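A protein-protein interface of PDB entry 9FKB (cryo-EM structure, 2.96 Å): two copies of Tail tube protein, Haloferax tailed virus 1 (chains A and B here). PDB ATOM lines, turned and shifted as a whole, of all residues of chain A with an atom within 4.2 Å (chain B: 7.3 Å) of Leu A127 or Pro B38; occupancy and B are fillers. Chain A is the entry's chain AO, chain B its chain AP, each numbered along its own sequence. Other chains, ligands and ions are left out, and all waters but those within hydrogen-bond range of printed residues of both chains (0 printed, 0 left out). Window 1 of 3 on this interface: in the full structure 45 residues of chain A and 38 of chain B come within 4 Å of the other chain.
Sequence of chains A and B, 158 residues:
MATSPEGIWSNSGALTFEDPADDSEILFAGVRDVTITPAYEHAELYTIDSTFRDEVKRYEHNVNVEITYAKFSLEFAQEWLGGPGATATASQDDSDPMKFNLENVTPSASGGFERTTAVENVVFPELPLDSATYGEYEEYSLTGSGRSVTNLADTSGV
The backbone NH (N) of Leu A129 is in hydrogen-bond range of the backbone carbonyl oxygen (O) of Ile B36, 2.8 Å away.
The backbone carbonyl oxygen (O) of Pro B38 is in hydrogen-bond range of the backbone NH (N) of Leu A127.
The backbone carbonyl oxygen (O) of Asn B64 is in hydrogen-bond range of the backbone NH (N) of Thr B37, at 2.9 Å.
O of Ala B39 sits at hydrogen-bond distance from ND1 of His B61 (3.1 Å).
N of Ala B39 is in hydrogen-bond range of O of Asn B62, 2.9 Å away.
Ala A77 touches Leu B152 (CB to CD2, 3.7 Å).
CH2 of Trp A80 touches O of Pro B38 (3.4 Å).
Trp A80 touches Tyr B40 (CH2 to CE1, 3.7 Å).
Glu A126 touches Thr B37 (CB to CG2, 3.9 Å).
Pro B38 touches Glu A126.
O of Leu A127 touches CA of Thr B37, 3.4 Å away.
Ile B36 touches Pro A128.
CA of Pro A128 touches OG1 of Thr B37 (3.9 Å).
Thr B117 touches Leu A129.
Leu A129 touches Leu B152 (CD2 to CD2, 3.6 Å).
Printed residues of chain B within 4 Å of Glu A126: Thr B37 (3.9 Å), Pro B38 (3.3 Å) and Ala B39 (3.5 Å).
Of the printed residues of chain A, Pro B38 touches Trp A80, Glu A126, Leu A127 and Leu A129.
Val B63 touches none of the printed residues of chain A.
Printed residues of chain A within 4 Å of Leu B152: Ala A77 and Leu A129.
The nearest printed residue of chain B that does not touch Trp A80 is Ala B39 (4.1 Å).
Printed residues of chain A that touch a printed residue of chain B: Ala A77, Trp A80, Glu A126, Leu A127, Pro A128 and Leu A129.
Hydrophobic or aromatic side chains of chain A within 4 Å of the printed part of chain B: Ala A77, Trp A80 and Leu A129.
Printed residues of chain B that touch a printed residue of chain A: Ile B36, Thr B37, Pro B38, Ala B39, Tyr B40, Thr B117 and Leu B152.
Hydrophobic or aromatic side chains of chain B that line the printed part of chain A: Pro B38, Ala B39, Tyr B40 and Leu B152.
Among the printed residues, 14 pairs touch across the chains.
Among the printed residues, no Asp or Glu carboxylate lies within 4 Å of a Lys or Arg side-chain nitrogen of the other chain.
No position is printed for both chains.
Of the 14 pairs that touch across the chains among the printed residues, none has its exchanged pair printed and touching as well.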
ATOM      1  N   PHE A  76      25.958 -34.198   0.880  1.00  0.00           N
ATOM      2  CA  PHE A  76      25.215 -33.618  -0.228  1.00  0.00           C
ATOM      3  C   PHE A  76      24.782 -32.187   0.066  1.00  0.00           C
ATOM      4  O   PHE A  76      24.947 -31.296  -0.764  1.00  0.00           O
ATOM      5  CB  PHE A  76      24.014 -34.501  -0.533  1.00  0.00           C
ATOM      6  CG  PHE A  76      23.115 -33.976  -1.619  1.00  0.00           C
ATOM      7  CD1 PHE A  76      23.397 -34.224  -2.961  1.00  0.00           C
ATOM      8  CD2 PHE A  76      21.988 -33.220  -1.309  1.00  0.00           C
ATOM      9  CE1 PHE A  76      22.574 -33.722  -3.967  1.00  0.00           C
ATOM     10  CE2 PHE A  76      21.165 -32.716  -2.319  1.00  0.00           C
ATOM     11  CZ  PHE A  76      21.456 -32.973  -3.648  1.00  0.00           C
ATOM     12  N   ALA A  77      24.266 -31.943   1.269  1.00  0.00           N
ATOM     13  CA  ALA A  77      23.879 -30.607   1.694  1.00  0.00           C
ATOM     14  C   ALA A  77      25.081 -29.660   1.739  1.00  0.00           C
ATOM     15  O   ALA A  77      24.983 -28.527   1.273  1.00  0.00           O
ATOM     16  CB  ALA A  77      23.171 -30.695   3.024  1.00  0.00           C
ATOM     17  N   TRP A  80      26.056 -28.699  -1.799  1.00  0.00           N
ATOM     18  CA  TRP A  80      25.114 -27.736  -2.357  1.00  0.00           C
ATOM     19  C   TRP A  80      25.331 -26.326  -1.806  1.00  0.00           C
ATOM     20  O   TRP A  80      25.276 -25.351  -2.548  1.00  0.00           O
ATOM     21  CB  TRP A  80      23.694 -28.212  -2.089  1.00  0.00           C
ATOM     22  CG  TRP A  80      22.621 -27.346  -2.659  1.00  0.00           C
ATOM     23  CD1 TRP A  80      22.027 -27.492  -3.882  1.00  0.00           C
ATOM     24  CD2 TRP A  80      22.016 -26.179  -2.052  1.00  0.00           C
ATOM     25  NE1 TRP A  80      21.085 -26.512  -4.053  1.00  0.00           N
ATOM     26  CE2 TRP A  80      21.036 -25.692  -2.952  1.00  0.00           C
ATOM     27  CE3 TRP A  80      22.178 -25.498  -0.840  1.00  0.00           C
ATOM     28  CZ2 TRP A  80      20.255 -24.556  -2.674  1.00  0.00           C
ATOM     29  CZ3 TRP A  80      21.415 -24.372  -0.565  1.00  0.00           C
ATOM     30  CH2 TRP A  80      20.448 -23.918  -1.465  1.00  0.00           C
ATOM     31  N   GLU A 126      16.518 -25.028  -4.770  1.00  0.00           N
ATOM     32  CA  GLU A 126      16.319 -25.030  -3.337  1.00  0.00           C
ATOM     33  C   GLU A 126      16.537 -26.426  -2.774  1.00  0.00           C
ATOM     34  O   GLU A 126      16.222 -27.424  -3.414  1.00  0.00           O
ATOM     35  CB  GLU A 126      14.943 -24.465  -3.006  1.00  0.00           C
ATOM     36  CG  GLU A 126      13.773 -25.241  -3.608  1.00  0.00           C
ATOM     37  CD  GLU A 126      12.463 -24.477  -3.805  1.00  0.00           C
ATOM     38  OE1 GLU A 126      12.516 -23.293  -4.220  1.00  0.00           O
ATOM     39  OE2 GLU A 126      11.383 -25.071  -3.548  1.00  0.00           O
ATOM     40  N   LEU A 127      17.081 -26.450  -1.557  1.00  0.00           N
ATOM     41  CA  LEU A 127      17.478 -27.662  -0.858  1.00  0.00           C
ATOM     42  C   LEU A 127      16.738 -27.696   0.472  1.00  0.00           C
ATOM     43  O   LEU A 127      16.881 -26.781   1.279  1.00  0.00           O
ATOM     44  CB  LEU A 127      18.985 -27.575  -0.605  1.00  0.00           C
ATOM     45  CG  LEU A 127      19.538 -28.598   0.384  1.00  0.00           C
ATOM     46  CD1 LEU A 127      19.631 -29.958  -0.296  1.00  0.00           C
ATOM     47  CD2 LEU A 127      20.921 -28.171   0.869  1.00  0.00           C
ATOM     48  N   PRO A 128      15.941 -28.744   0.779  1.00  0.00           N
ATOM     49  CA  PRO A 128      15.398 -28.880   2.128  1.00  0.00           C
ATOM     50  C   PRO A 128      16.501 -29.379   3.058  1.00  0.00           C
ATOM     51  O   PRO A 128      17.252 -30.305   2.735  1.00  0.00           O
ATOM     52  CB  PRO A 128      14.269 -29.897   1.956  1.00  0.00           C
ATOM     53  CG  PRO A 128      14.791 -30.769   0.824  1.00  0.00           C
ATOM     54  CD  PRO A 128      15.506 -29.816  -0.116  1.00  0.00           C
ATOM     55  N   LEU A 129      16.584 -28.755   4.243  1.00  0.00           N
ATOM     56  CA  LEU A 129      17.431 -29.250   5.316  1.00  0.00           C
ATOM     57  C   LEU A 129      16.580 -30.018   6.321  1.00  0.00           C
ATOM     58  O   LEU A 129      16.622 -31.243   6.345  1.00  0.00           O
ATOM     59  CB  LEU A 129      18.168 -28.088   5.974  1.00  0.00           C
ATOM     60  CG  LEU A 129      19.229 -27.444   5.082  1.00  0.00           C
ATOM     61  CD1 LEU A 129      19.984 -26.401   5.899  1.00  0.00           C
ATOM     62  CD2 LEU A 129      20.206 -28.464   4.466  1.00  0.00           C
ATOM     63  N   ILE B  36      12.673 -26.346   6.828  1.00  0.00           N
ATOM     64  CA  ILE B  36      13.698 -25.342   6.599  1.00  0.00           C
ATOM     65  C   ILE B  36      14.309 -25.616   5.228  1.00  0.00           C
ATOM     66  O   ILE B  36      14.850 -26.697   4.984  1.00  0.00           O
ATOM     67  CB  ILE B  36      14.772 -25.393   7.702  1.00  0.00           C
ATOM     68  CG1 ILE B  36      14.145 -25.052   9.047  1.00  0.00           C
ATOM     69  CG2 ILE B  36      15.955 -24.472   7.400  1.00  0.00           C
ATOM     70  CD1 ILE B  36      15.148 -24.920  10.177  1.00  0.00           C
ATOM     71  N   THR B  37      14.242 -24.626   4.332  1.00  0.00           N
ATOM     72  CA  THR B  37      14.638 -24.825   2.945  1.00  0.00           C
ATOM     73  C   THR B  37      15.425 -23.626   2.435  1.00  0.00           C
ATOM     74  O   THR B  37      14.848 -22.638   1.992  1.00  0.00           O
ATOM     75  CB  THR B  37      13.407 -25.019   2.052  1.00  0.00           C
ATOM     76  OG1 THR B  37      12.653 -26.135   2.522  1.00  0.00           O
ATOM     77  CG2 THR B  37      13.768 -25.342   0.616  1.00  0.00           C
ATOM     78  N   PRO B  38      16.769 -23.648   2.519  1.00  0.00           N
ATOM     79  CA  PRO B  38      17.620 -22.740   1.764  1.00  0.00           C
ATOM     80  C   PRO B  38      17.314 -22.779   0.270  1.00  0.00           C
ATOM     81  O   PRO B  38      17.192 -23.839  -0.337  1.00  0.00           O
ATOM     82  CB  PRO B  38      19.017 -23.320   2.017  1.00  0.00           C
ATOM     83  CG  PRO B  38      18.904 -23.828   3.417  1.00  0.00           C
ATOM     84  CD  PRO B  38      17.552 -24.506   3.399  1.00  0.00           C
ATOM     85  N   ALA B  39      17.217 -21.592  -0.322  1.00  0.00           N
ATOM     86  CA  ALA B  39      16.836 -21.445  -1.713  1.00  0.00           C
ATOM     87  C   ALA B  39      17.598 -20.292  -2.358  1.00  0.00           C
ATOM     88  O   ALA B  39      18.036 -19.365  -1.690  1.00  0.00           O
ATOM     89  CB  ALA B  39      15.367 -21.168  -1.788  1.00  0.00           C
ATOM     90  N   TYR B  40      17.748 -20.386  -3.678  1.00  0.00           N
ATOM     91  CA  TYR B  40      18.182 -19.280  -4.508  1.00  0.00           C
ATOM     92  C   TYR B  40      17.290 -19.218  -5.739  1.00  0.00           C
ATOM     93  O   TYR B  40      16.778 -20.235  -6.204  1.00  0.00           O
ATOM     94  CB  TYR B  40      19.597 -19.530  -5.007  1.00  0.00           C
ATOM     95  CG  TYR B  40      20.721 -19.532  -3.997  1.00  0.00           C
ATOM     96  CD1 TYR B  40      21.043 -20.687  -3.315  1.00  0.00           C
ATOM     97  CD2 TYR B  40      21.547 -18.430  -3.815  1.00  0.00           C
ATOM     98  CE1 TYR B  40      22.148 -20.741  -2.480  1.00  0.00           C
ATOM     99  CE2 TYR B  40      22.681 -18.481  -3.008  1.00  0.00           C
ATOM    100  CZ  TYR B  40      22.997 -19.653  -2.347  1.00  0.00           C
ATOM    101  OH  TYR B  40      24.109 -19.754  -1.557  1.00  0.00           O
ATOM    102  N   HIS B  61      19.544 -15.415  -2.342  1.00  0.00           N
ATOM    103  CA  HIS B  61      19.473 -16.398  -1.290  1.00  0.00           C
ATOM    104  C   HIS B  61      18.424 -15.977  -0.265  1.00  0.00           C
ATOM    105  O   HIS B  61      18.362 -14.819   0.142  1.00  0.00           O
ATOM    106  CB  HIS B  61      20.840 -16.514  -0.640  1.00  0.00           C
ATOM    107  CG  HIS B  61      20.910 -17.690   0.264  1.00  0.00           C
ATOM    108  ND1 HIS B  61      20.741 -18.990  -0.156  1.00  0.00           N
ATOM    109  CD2 HIS B  61      21.062 -17.722   1.607  1.00  0.00           C
ATOM    110  CE1 HIS B  61      20.835 -19.786   0.905  1.00  0.00           C
ATOM    111  NE2 HIS B  61      21.040 -19.025   2.002  1.00  0.00           N
ATOM    112  N   ASN B  62      17.631 -16.951   0.171  1.00  0.00           N
ATOM    113  CA  ASN B  62      16.874 -16.848   1.409  1.00  0.00           C
ATOM    114  C   ASN B  62      16.647 -18.253   1.958  1.00  0.00           C
ATOM    115  O   ASN B  62      16.820 -19.242   1.251  1.00  0.00           O
ATOM    116  CB  ASN B  62      15.581 -16.051   1.232  1.00  0.00           C
ATOM    117  CG  ASN B  62      14.448 -16.869   0.655  1.00  0.00           C
ATOM    118  OD1 ASN B  62      14.627 -17.636  -0.295  1.00  0.00           O
ATOM    119  ND2 ASN B  62      13.250 -16.743   1.222  1.00  0.00           N
ATOM    120  N   VAL B  63      16.259 -18.358   3.225  1.00  0.00           N
ATOM    121  CA  VAL B  63      15.851 -19.633   3.782  1.00  0.00           C
ATOM    122  C   VAL B  63      14.358 -19.571   4.048  1.00  0.00           C
ATOM    123  O   VAL B  63      13.927 -18.793   4.882  1.00  0.00           O
ATOM    124  CB  VAL B  63      16.614 -19.913   5.085  1.00  0.00           C
ATOM    125  CG1 VAL B  63      16.259 -21.282   5.620  1.00  0.00           C
ATOM    126  CG2 VAL B  63      18.108 -19.863   4.874  1.00  0.00           C
ATOM    127  N   ASN B  64      13.572 -20.390   3.354  1.00  0.00           N
ATOM    128  CA  ASN B  64      12.162 -20.522   3.680  1.00  0.00           C
ATOM    129  C   ASN B  64      12.022 -21.329   4.968  1.00  0.00           C
ATOM    130  O   ASN B  64      12.550 -22.430   5.053  1.00  0.00           O
ATOM    131  CB  ASN B  64      11.396 -21.167   2.526  1.00  0.00           C
ATOM    132  CG  ASN B  64      11.435 -20.336   1.256  1.00  0.00           C
ATOM    133  OD1 ASN B  64      11.424 -19.102   1.278  1.00  0.00           O
ATOM    134  ND2 ASN B  64      11.466 -21.023   0.124  1.00  0.00           N
ATOM    135  N   VAL B  65      11.349 -20.762   5.969  1.00  0.00           N
ATOM    136  CA  VAL B  65      11.056 -21.442   7.216  1.00  0.00           C
ATOM    137  C   VAL B  65       9.545 -21.555   7.369  1.00  0.00           C
ATOM    138  O   VAL B  65       8.855 -20.550   7.363  1.00  0.00           O
ATOM    139  CB  VAL B  65      11.647 -20.690   8.415  1.00  0.00           C
ATOM    140  CG1 VAL B  65      11.344 -21.411   9.717  1.00  0.00           C
ATOM    141  CG2 VAL B  65      13.146 -20.527   8.293  1.00  0.00           C
ATOM    142  N   THR B 117      21.169 -27.349  12.491  1.00  0.00           N
ATOM    143  CA  THR B 117      20.801 -26.384  11.470  1.00  0.00           C
ATOM    144  C   THR B 117      20.544 -25.048  12.168  1.00  0.00           C
ATOM    145  O   THR B 117      19.743 -24.994  13.087  1.00  0.00           O
ATOM    146  CB  THR B 117      19.517 -26.817  10.745  1.00  0.00           C
ATOM    147  OG1 THR B 117      19.569 -28.160  10.251  1.00  0.00           O
ATOM    148  CG2 THR B 117      19.180 -25.889   9.606  1.00  0.00           C
ATOM    149  N   VAL B 119      19.857 -20.661  11.442  1.00  0.00           N
ATOM    150  CA  VAL B 119      19.400 -19.715  10.431  1.00  0.00           C
ATOM    151  C   VAL B 119      19.368 -18.316  11.041  1.00  0.00           C
ATOM    152  O   VAL B 119      18.784 -18.115  12.105  1.00  0.00           O
ATOM    153  CB  VAL B 119      17.999 -20.100   9.919  1.00  0.00           C
ATOM    154  CG1 VAL B 119      17.528 -19.130   8.842  1.00  0.00           C
ATOM    155  CG2 VAL B 119      17.943 -21.521   9.354  1.00  0.00           C
ATOM    156  N   SER B 148      20.096 -16.277   5.847  1.00  0.00           N
ATOM    157  CA  SER B 148      21.038 -17.307   5.421  1.00  0.00           C
ATOM    158  C   SER B 148      21.173 -18.395   6.488  1.00  0.00           C
ATOM    159  O   SER B 148      20.732 -18.225   7.618  1.00  0.00           O
ATOM    160  CB  SER B 148      22.389 -16.701   5.105  1.00  0.00           C
ATOM    161  OG  SER B 148      23.082 -16.285   6.278  1.00  0.00           O
ATOM    162  N   VAL B 149      21.782 -19.533   6.114  1.00  0.00           N
ATOM    163  CA  VAL B 149      22.172 -20.567   7.066  1.00  0.00           C
ATOM    164  C   VAL B 149      23.535 -20.221   7.658  1.00  0.00           C
ATOM    165  O   VAL B 149      24.531 -20.170   6.936  1.00  0.00           O
ATOM    166  CB  VAL B 149      22.233 -21.942   6.389  1.00  0.00           C
ATOM    167  CG1 VAL B 149      22.764 -23.030   7.321  1.00  0.00           C
ATOM    168  CG2 VAL B 149      20.863 -22.320   5.872  1.00  0.00           C
ATOM    169  N   LEU B 152      25.421 -25.544   9.435  1.00  0.00           N
ATOM    170  CA  LEU B 152      24.967 -26.878   9.084  1.00  0.00           C
ATOM    171  C   LEU B 152      26.167 -27.820   9.160  1.00  0.00           C
ATOM    172  O   LEU B 152      26.971 -27.905   8.224  1.00  0.00           O
ATOM    173  CB  LEU B 152      24.380 -26.887   7.675  1.00  0.00           C
ATOM    174  CG  LEU B 152      23.948 -28.274   7.227  1.00  0.00           C
ATOM    175  CD1 LEU B 152      22.801 -28.767   8.102  1.00  0.00           C
ATOM    176  CD2 LEU B 152      23.562 -28.253   5.761  1.00  0.00           C
